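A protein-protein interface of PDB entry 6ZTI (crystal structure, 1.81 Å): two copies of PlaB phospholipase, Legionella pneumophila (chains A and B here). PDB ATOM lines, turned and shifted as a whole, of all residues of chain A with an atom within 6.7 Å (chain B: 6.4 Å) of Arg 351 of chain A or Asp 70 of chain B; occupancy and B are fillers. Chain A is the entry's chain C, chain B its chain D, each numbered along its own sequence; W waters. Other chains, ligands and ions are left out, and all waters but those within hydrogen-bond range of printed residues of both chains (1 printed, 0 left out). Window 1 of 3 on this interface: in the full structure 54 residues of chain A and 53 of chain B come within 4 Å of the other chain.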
ATOM      1  N   ILE A 348      -4.622   9.652 -17.279  1.00  0.00           N
ATOM      2  CA  ILE A 348      -3.350   9.022 -17.605  1.00  0.00           C
ATOM      3  C   ILE A 348      -3.584   7.521 -17.685  1.00  0.00           C
ATOM      4  O   ILE A 348      -4.665   7.029 -17.359  1.00  0.00           O
ATOM      5  CB  ILE A 348      -2.262   9.336 -16.559  1.00  0.00           C
ATOM      6  CG1 ILE A 348      -2.698   8.837 -15.176  1.00  0.00           C
ATOM      7  CG2 ILE A 348      -2.000  10.830 -16.518  1.00  0.00           C
ATOM      8  CD1 ILE A 348      -1.661   9.041 -14.089  1.00  0.00           C
ATOM      9  N   ASP A 349      -2.559   6.790 -18.136  1.00  0.00           N
ATOM     10  CA  ASP A 349      -2.542   5.326 -18.063  1.00  0.00           C
ATOM     11  C   ASP A 349      -1.313   4.855 -17.289  1.00  0.00           C
ATOM     12  O   ASP A 349      -0.484   5.649 -16.853  1.00  0.00           O
ATOM     13  CB  ASP A 349      -2.633   4.689 -19.458  1.00  0.00           C
ATOM     14  CG  ASP A 349      -1.336   4.768 -20.268  1.00  0.00           C
ATOM     15  OD1 ASP A 349      -0.270   5.149 -19.732  1.00  0.00           O
ATOM     16  OD2 ASP A 349      -1.397   4.426 -21.478  1.00  0.00           O
ATOM     17  N   ASP A 350      -1.223   3.539 -17.095  1.00  0.00           N
ATOM     18  CA  ASP A 350      -0.183   2.930 -16.285  1.00  0.00           C
ATOM     19  C   ASP A 350       1.128   2.750 -17.034  1.00  0.00           C
ATOM     20  O   ASP A 350       2.012   2.052 -16.529  1.00  0.00           O
ATOM     21  CB  ASP A 350      -0.650   1.575 -15.756  1.00  0.00           C
ATOM     22  CG  ASP A 350      -0.990   0.589 -16.868  1.00  0.00           C
ATOM     23  OD1 ASP A 350      -1.245   1.022 -18.015  1.00  0.00           O
ATOM     24  OD2 ASP A 350      -1.016  -0.627 -16.585  1.00  0.00           O
ATOM     25  N   ARG A 351       1.278   3.351 -18.219  1.00  0.00           N
ATOM     26  CA  ARG A 351       2.538   3.312 -18.956  1.00  0.00           C
ATOM     27  C   ARG A 351       3.120   4.710 -19.157  1.00  0.00           C
ATOM     28  O   ARG A 351       3.980   4.901 -20.024  1.00  0.00           O
ATOM     29  CB  ARG A 351       2.369   2.618 -20.317  1.00  0.00           C
ATOM     30  CG  ARG A 351       1.793   1.211 -20.262  1.00  0.00           C
ATOM     31  CD  ARG A 351       2.584   0.319 -19.345  1.00  0.00           C
ATOM     32  NE  ARG A 351       3.955   0.133 -19.804  1.00  0.00           N
ATOM     33  CZ  ARG A 351       4.943  -0.373 -19.064  1.00  0.00           C
ATOM     34  NH1 ARG A 351       4.726  -0.740 -17.806  1.00  0.00           N
ATOM     35  NH2 ARG A 351       6.159  -0.505 -19.582  1.00  0.00           N
ATOM     36  N   GLY A 352       2.657   5.698 -18.395  1.00  0.00           N
ATOM     37  CA  GLY A 352       3.220   7.032 -18.453  1.00  0.00           C
ATOM     38  C   GLY A 352       2.626   7.951 -19.497  1.00  0.00           C
ATOM     39  O   GLY A 352       3.213   9.004 -19.771  1.00  0.00           O
ATOM     40  N   ASN A 353       1.480   7.606 -20.075  1.00  0.00           N
ATOM     41  CA  ASN A 353       0.844   8.417 -21.102  1.00  0.00           C
ATOM     42  C   ASN A 353      -0.242   9.276 -20.488  1.00  0.00           C
ATOM     43  O   ASN A 353      -0.991   8.815 -19.626  1.00  0.00           O
ATOM     44  CB  ASN A 353       0.233   7.541 -22.196  1.00  0.00           C
ATOM     45  CG  ASN A 353       1.265   6.717 -22.923  1.00  0.00           C
ATOM     46  OD1 ASN A 353       1.233   5.481 -22.891  1.00  0.00           O
ATOM     47  ND2 ASN A 353       2.202   7.398 -23.577  1.00  0.00           N
ATOM     48  N   MET A 458      -6.245   6.859 -13.522  1.00  0.00           N
ATOM     49  CA  MET A 458      -5.242   6.066 -14.232  1.00  0.00           C
ATOM     50  C   MET A 458      -5.914   4.806 -14.773  1.00  0.00           C
ATOM     51  O   MET A 458      -6.346   3.940 -14.000  1.00  0.00           O
ATOM     52  CB  MET A 458      -4.070   5.713 -13.321  1.00  0.00           C
ATOM     53  CG  MET A 458      -2.960   4.926 -14.037  1.00  0.00           C
ATOM     54  SD  MET A 458      -1.660   4.316 -12.971  1.00  0.00           S
ATOM     55  CE  MET A 458      -0.592   5.749 -12.952  1.00  0.00           C
ATOM     56  N   LEU A 459      -5.993   4.701 -16.101  1.00  0.00           N
ATOM     57  CA  LEU A 459      -6.512   3.509 -16.760  1.00  0.00           C
ATOM     58  C   LEU A 459      -5.392   2.511 -17.035  1.00  0.00           C
ATOM     59  O   LEU A 459      -4.224   2.879 -17.185  1.00  0.00           O
ATOM     60  CB  LEU A 459      -7.191   3.878 -18.067  1.00  0.00           C
ATOM     61  CG  LEU A 459      -8.366   4.843 -17.983  1.00  0.00           C
ATOM     62  CD1 LEU A 459      -8.899   5.039 -19.371  1.00  0.00           C
ATOM     63  CD2 LEU A 459      -9.439   4.303 -17.060  1.00  0.00           C
ATOM     64  N   ARG A 461      -3.565   0.265 -19.611  1.00  0.00           N
ATOM     65  CA  ARG A 461      -3.351   0.098 -21.043  1.00  0.00           C
ATOM     66  C   ARG A 461      -3.375  -1.398 -21.343  1.00  0.00           C
ATOM     67  O   ARG A 461      -2.504  -2.140 -20.882  1.00  0.00           O
ATOM     68  CB  ARG A 461      -2.031   0.737 -21.448  1.00  0.00           C
ATOM     69  CG  ARG A 461      -1.789   0.750 -22.942  1.00  0.00           C
ATOM     70  CD  ARG A 461      -0.617   1.638 -23.289  1.00  0.00           C
ATOM     71  NE  ARG A 461      -0.250   1.515 -24.696  1.00  0.00           N
ATOM     72  CZ  ARG A 461      -0.772   2.247 -25.676  1.00  0.00           C
ATOM     73  NH1 ARG A 461      -1.690   3.169 -25.412  1.00  0.00           N
ATOM     74  NH2 ARG A 461      -0.366   2.058 -26.927  1.00  0.00           N
ATOM     75  N   VAL A 463      -3.076  -4.445 -23.958  1.00  0.00           N
ATOM     76  CA  VAL A 463      -2.401  -4.762 -25.210  1.00  0.00           C
ATOM     77  C   VAL A 463      -2.719  -6.213 -25.529  1.00  0.00           C
ATOM     78  O   VAL A 463      -2.451  -7.105 -24.713  1.00  0.00           O
ATOM     79  CB  VAL A 463      -0.886  -4.533 -25.110  1.00  0.00           C
ATOM     80  CG1 VAL A 463      -0.186  -4.810 -26.444  1.00  0.00           C
ATOM     81  CG2 VAL A 463      -0.603  -3.116 -24.623  1.00  0.00           C
ATOM     82  N   ILE A 488      -1.889  -9.122 -22.800  1.00  0.00           N
ATOM     83  CA  ILE A 488      -0.619  -9.461 -22.167  1.00  0.00           C
ATOM     84  C   ILE A 488      -0.651  -9.028 -20.705  1.00  0.00           C
ATOM     85  O   ILE A 488      -1.416  -8.145 -20.300  1.00  0.00           O
ATOM     86  CB  ILE A 488       0.567  -8.809 -22.904  1.00  0.00           C
ATOM     87  CG1 ILE A 488       0.596  -7.293 -22.649  1.00  0.00           C
ATOM     88  CG2 ILE A 488       0.492  -9.097 -24.400  1.00  0.00           C
ATOM     89  CD1 ILE A 488       1.609  -6.524 -23.500  1.00  0.00           C
ATOM     90  N   THR B  68       2.891   1.049 -29.397  1.00  0.00           N
ATOM     91  CA  THR B  68       4.173   1.659 -29.081  1.00  0.00           C
ATOM     92  C   THR B  68       5.269   0.600 -28.971  1.00  0.00           C
ATOM     93  O   THR B  68       5.010  -0.605 -28.873  1.00  0.00           O
ATOM     94  CB  THR B  68       4.072   2.434 -27.769  1.00  0.00           C
ATOM     95  OG1 THR B  68       3.864   1.506 -26.697  1.00  0.00           O
ATOM     96  CG2 THR B  68       2.917   3.419 -27.812  1.00  0.00           C
ATOM     97  N   VAL B  69       6.521   1.070 -28.973  1.00  0.00           N
ATOM     98  CA  VAL B  69       7.652   0.160 -28.787  1.00  0.00           C
ATOM     99  C   VAL B  69       7.596  -0.464 -27.403  1.00  0.00           C
ATOM    100  O   VAL B  69       7.882  -1.658 -27.221  1.00  0.00           O
ATOM    101  CB  VAL B  69       8.977   0.906 -29.020  1.00  0.00           C
ATOM    102  CG1 VAL B  69      10.146   0.061 -28.582  1.00  0.00           C
ATOM    103  CG2 VAL B  69       9.110   1.270 -30.475  1.00  0.00           C
ATOM    104  N   ASP B  70       7.220   0.332 -26.407  1.00  0.00           N
ATOM    105  CA  ASP B  70       6.922  -0.216 -25.086  1.00  0.00           C
ATOM    106  C   ASP B  70       5.923  -1.365 -25.183  1.00  0.00           C
ATOM    107  O   ASP B  70       6.165  -2.457 -24.652  1.00  0.00           O
ATOM    108  CB  ASP B  70       6.383   0.896 -24.192  1.00  0.00           C
ATOM    109  CG  ASP B  70       6.021   0.415 -22.817  1.00  0.00           C
ATOM    110  OD1 ASP B  70       6.952   0.068 -22.055  1.00  0.00           O
ATOM    111  OD2 ASP B  70       4.805   0.393 -22.505  1.00  0.00           O
ATOM    112  N   ASP B  71       4.780  -1.130 -25.851  1.00  0.00           N
ATOM    113  CA  ASP B  71       3.788  -2.190 -26.064  1.00  0.00           C
ATOM    114  C   ASP B  71       4.421  -3.442 -26.672  1.00  0.00           C
ATOM    115  O   ASP B  71       4.168  -4.563 -26.214  1.00  0.00           O
ATOM    116  CB  ASP B  71       2.649  -1.728 -26.987  1.00  0.00           C
ATOM    117  CG  ASP B  71       1.832  -0.551 -26.445  1.00  0.00           C
ATOM    118  OD1 ASP B  71       1.745  -0.322 -25.218  1.00  0.00           O
ATOM    119  OD2 ASP B  71       1.233   0.150 -27.298  1.00  0.00           O
ATOM    120  N   ILE B  72       5.219  -3.279 -27.736  1.00  0.00           N
ATOM    121  CA  ILE B  72       5.769  -4.447 -28.420  1.00  0.00           C
ATOM    122  C   ILE B  72       6.730  -5.198 -27.505  1.00  0.00           C
ATOM    123  O   ILE B  72       6.732  -6.430 -27.471  1.00  0.00           O
ATOM    124  CB  ILE B  72       6.456  -4.043 -29.741  1.00  0.00           C
ATOM    125  CG1 ILE B  72       5.442  -3.383 -30.695  1.00  0.00           C
ATOM    126  CG2 ILE B  72       7.048  -5.251 -30.416  1.00  0.00           C
ATOM    127  CD1 ILE B  72       6.076  -2.611 -31.827  1.00  0.00           C
ATOM    128  N   ALA B  73       7.589  -4.470 -26.777  1.00  0.00           N
ATOM    129  CA  ALA B  73       8.556  -5.112 -25.890  1.00  0.00           C
ATOM    130  C   ALA B  73       7.857  -5.875 -24.766  1.00  0.00           C
ATOM    131  O   ALA B  73       8.293  -6.968 -24.384  1.00  0.00           O
ATOM    132  CB  ALA B  73       9.518  -4.061 -25.322  1.00  0.00           C
ATOM    133  N   ARG B  74       6.770  -5.315 -24.225  1.00  0.00           N
ATOM    134  CA  ARG B  74       5.972  -6.034 -23.231  1.00  0.00           C
ATOM    135  C   ARG B  74       5.330  -7.277 -23.841  1.00  0.00           C
ATOM    136  O   ARG B  74       5.188  -8.309 -23.173  1.00  0.00           O
ATOM    137  CB  ARG B  74       4.867  -5.132 -22.673  1.00  0.00           C
ATOM    138  CG  ARG B  74       5.301  -4.016 -21.746  1.00  0.00           C
ATOM    139  CD  ARG B  74       4.087  -3.161 -21.316  1.00  0.00           C
ATOM    140  NE  ARG B  74       3.017  -3.969 -20.717  1.00  0.00           N
ATOM    141  CZ  ARG B  74       1.752  -3.573 -20.553  1.00  0.00           C
ATOM    142  NH1 ARG B  74       1.356  -2.370 -20.951  1.00  0.00           N
ATOM    143  NH2 ARG B  74       0.866  -4.388 -19.993  1.00  0.00           N
ATOM    144  N   ALA B  75       4.899  -7.177 -25.103  1.00  0.00           N
ATOM    145  CA  ALA B  75       4.241  -8.303 -25.758  1.00  0.00           C
ATOM    146  C   ALA B  75       5.221  -9.424 -26.063  1.00  0.00           C
ATOM    147  O   ALA B  75       4.833 -10.595 -26.075  1.00  0.00           O
ATOM    148  CB  ALA B  75       3.560  -7.839 -27.044  1.00  0.00           C
ATOM    149  N   LYS B 108      14.863  -2.801 -25.647  1.00  0.00           N
ATOM    150  CA  LYS B 108      13.881  -2.239 -24.721  1.00  0.00           C
ATOM    151  C   LYS B 108      13.318  -3.314 -23.797  1.00  0.00           C
ATOM    152  O   LYS B 108      13.106  -3.069 -22.599  1.00  0.00           O
ATOM    153  CB  LYS B 108      12.751  -1.566 -25.507  1.00  0.00           C
ATOM    154  CG  LYS B 108      11.608  -1.026 -24.661  1.00  0.00           C
ATOM    155  CD  LYS B 108      12.023   0.190 -23.824  1.00  0.00           C
ATOM    156  CE  LYS B 108      10.832   0.753 -23.042  1.00  0.00           C
ATOM    157  NZ  LYS B 108      11.229   1.717 -21.974  1.00  0.00           N
ATOM    158  N   LEU B 112      13.314  -3.213 -19.828  1.00  0.00           N
ATOM    159  CA  LEU B 112      12.087  -3.222 -19.038  1.00  0.00           C
ATOM    160  C   LEU B 112      12.093  -4.310 -17.980  1.00  0.00           C
ATOM    161  O   LEU B 112      11.490  -4.133 -16.913  1.00  0.00           O
ATOM    162  CB  LEU B 112      10.869  -3.420 -19.943  1.00  0.00           C
ATOM    163  CG  LEU B 112      10.337  -2.225 -20.728  1.00  0.00           C
ATOM    164  CD1 LEU B 112       9.378  -2.716 -21.775  1.00  0.00           C
ATOM    165  CD2 LEU B 112       9.657  -1.225 -19.815  1.00  0.00           C
ATOM    166  N   TRP B 165       9.407   6.774 -32.231  1.00  0.00           N
ATOM    167  CA  TRP B 165      10.614   6.197 -31.647  1.00  0.00           C
ATOM    168  C   TRP B 165      11.771   6.266 -32.627  1.00  0.00           C
ATOM    169  O   TRP B 165      12.892   6.629 -32.258  1.00  0.00           O
ATOM    170  CB  TRP B 165      10.369   4.731 -31.233  1.00  0.00           C
ATOM    171  CG  TRP B 165      11.410   4.209 -30.280  1.00  0.00           C
ATOM    172  CD1 TRP B 165      11.288   4.085 -28.924  1.00  0.00           C
ATOM    173  CD2 TRP B 165      12.742   3.778 -30.602  1.00  0.00           C
ATOM    174  NE1 TRP B 165      12.451   3.609 -28.387  1.00  0.00           N
ATOM    175  CE2 TRP B 165      13.362   3.410 -29.389  1.00  0.00           C
ATOM    176  CE3 TRP B 165      13.466   3.673 -31.790  1.00  0.00           C
ATOM    177  CZ2 TRP B 165      14.667   2.945 -29.329  1.00  0.00           C
ATOM    178  CZ3 TRP B 165      14.776   3.212 -31.733  1.00  0.00           C
ATOM    179  CH2 TRP B 165      15.360   2.849 -30.507  1.00  0.00           C
HETATM  180  O   HOH W   1       3.101   1.978 -24.184  1.00  0.00           O
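No position is printed for both chains.
Hydrophobic or aromatic side chains of chain A within 4 Å of the printed part of chain B: Val 463 and Ile 488.
Of the 11 printed residues of chain B, 6 touch a printed residue of chain A.
Along chain B the printed residues that touch a printed residue of chain A span positions 68 to 112.
N of Arg 351 of chain A is in hydrogen-bond range of OD1 of Asp 349 of chain A (2.8 Å).
The side-chain carboxylate of Asp 350 of chain A sits at hydrogen-bond distance from the backbone NH of Arg 461 of chain A, at 2.9 Å.
O of Val 463 of chain A lies within hydrogen-bond range of N of Ile 488 of chain A (2.8 Å).
The backbone NH (N) of Thr 68 of chain B sits at hydrogen-bond distance from the side-chain carboxylate (OD2) of Asp 71 of chain B (2.8 Å).
Water W1 lies within hydrogen-bond range of the side-chain hydroxyl (OG1) of Thr 68 of chain B, the side-chain carboxylate (OD1) of Asp 71 of chain B, the side-chain carboxylate (OD2) of Asp 70 of chain B and the guanidinium group (NE) of Arg 461 of chain A.
Arg 351 of chain A touches just these residues of chain B: Asp 70 (2.7 Å), Arg 74 (3.4 Å) and Leu 112 (3.6 Å).
Of the printed residues of chain B, Val 463 of chain A touches Asp 71.
Of the printed residues of chain A, Ala 75 of chain B touches Ile 488.
Of the printed residues of chain B, Arg 461 of chain A touches Thr 68 (3.7 Å), Asp 71 (2.5 Å) and Arg 74 (3.9 Å).
The nearest residue of chain B that does not touch Arg 351 of chain A is Asp 71 of chain B (5.2 Å).
The nearest printed residue of chain A that does not touch Leu 112 of chain B is Ile 488 of chain A (8.8 Å).
Among the printed residues, pairs that only touch across the chains: Arg 351 of chain A with Arg 74 of chain B, Arg 351 of chain A with Leu 112 of chain B, Ile 488 of chain A with Arg 74 of chain B, Arg 461 of chain A with Thr 68 of chain B, Val 463 of chain A with Asp 71 of chain B, Ile 488 of chain A with Ala 75 of chain B and Arg 461 of chain A with Arg 74 of chain B.
The guanidinium group (NH2) of Arg 351 of chain A lies within salt-bridge range of the side-chain carboxylate (OD1) of Asp 70 of chain B (2.7 Å).
NH2 of Arg 461 of chain A is in salt-bridge range of OD2 of Asp 71 of chain B (2.5 Å).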
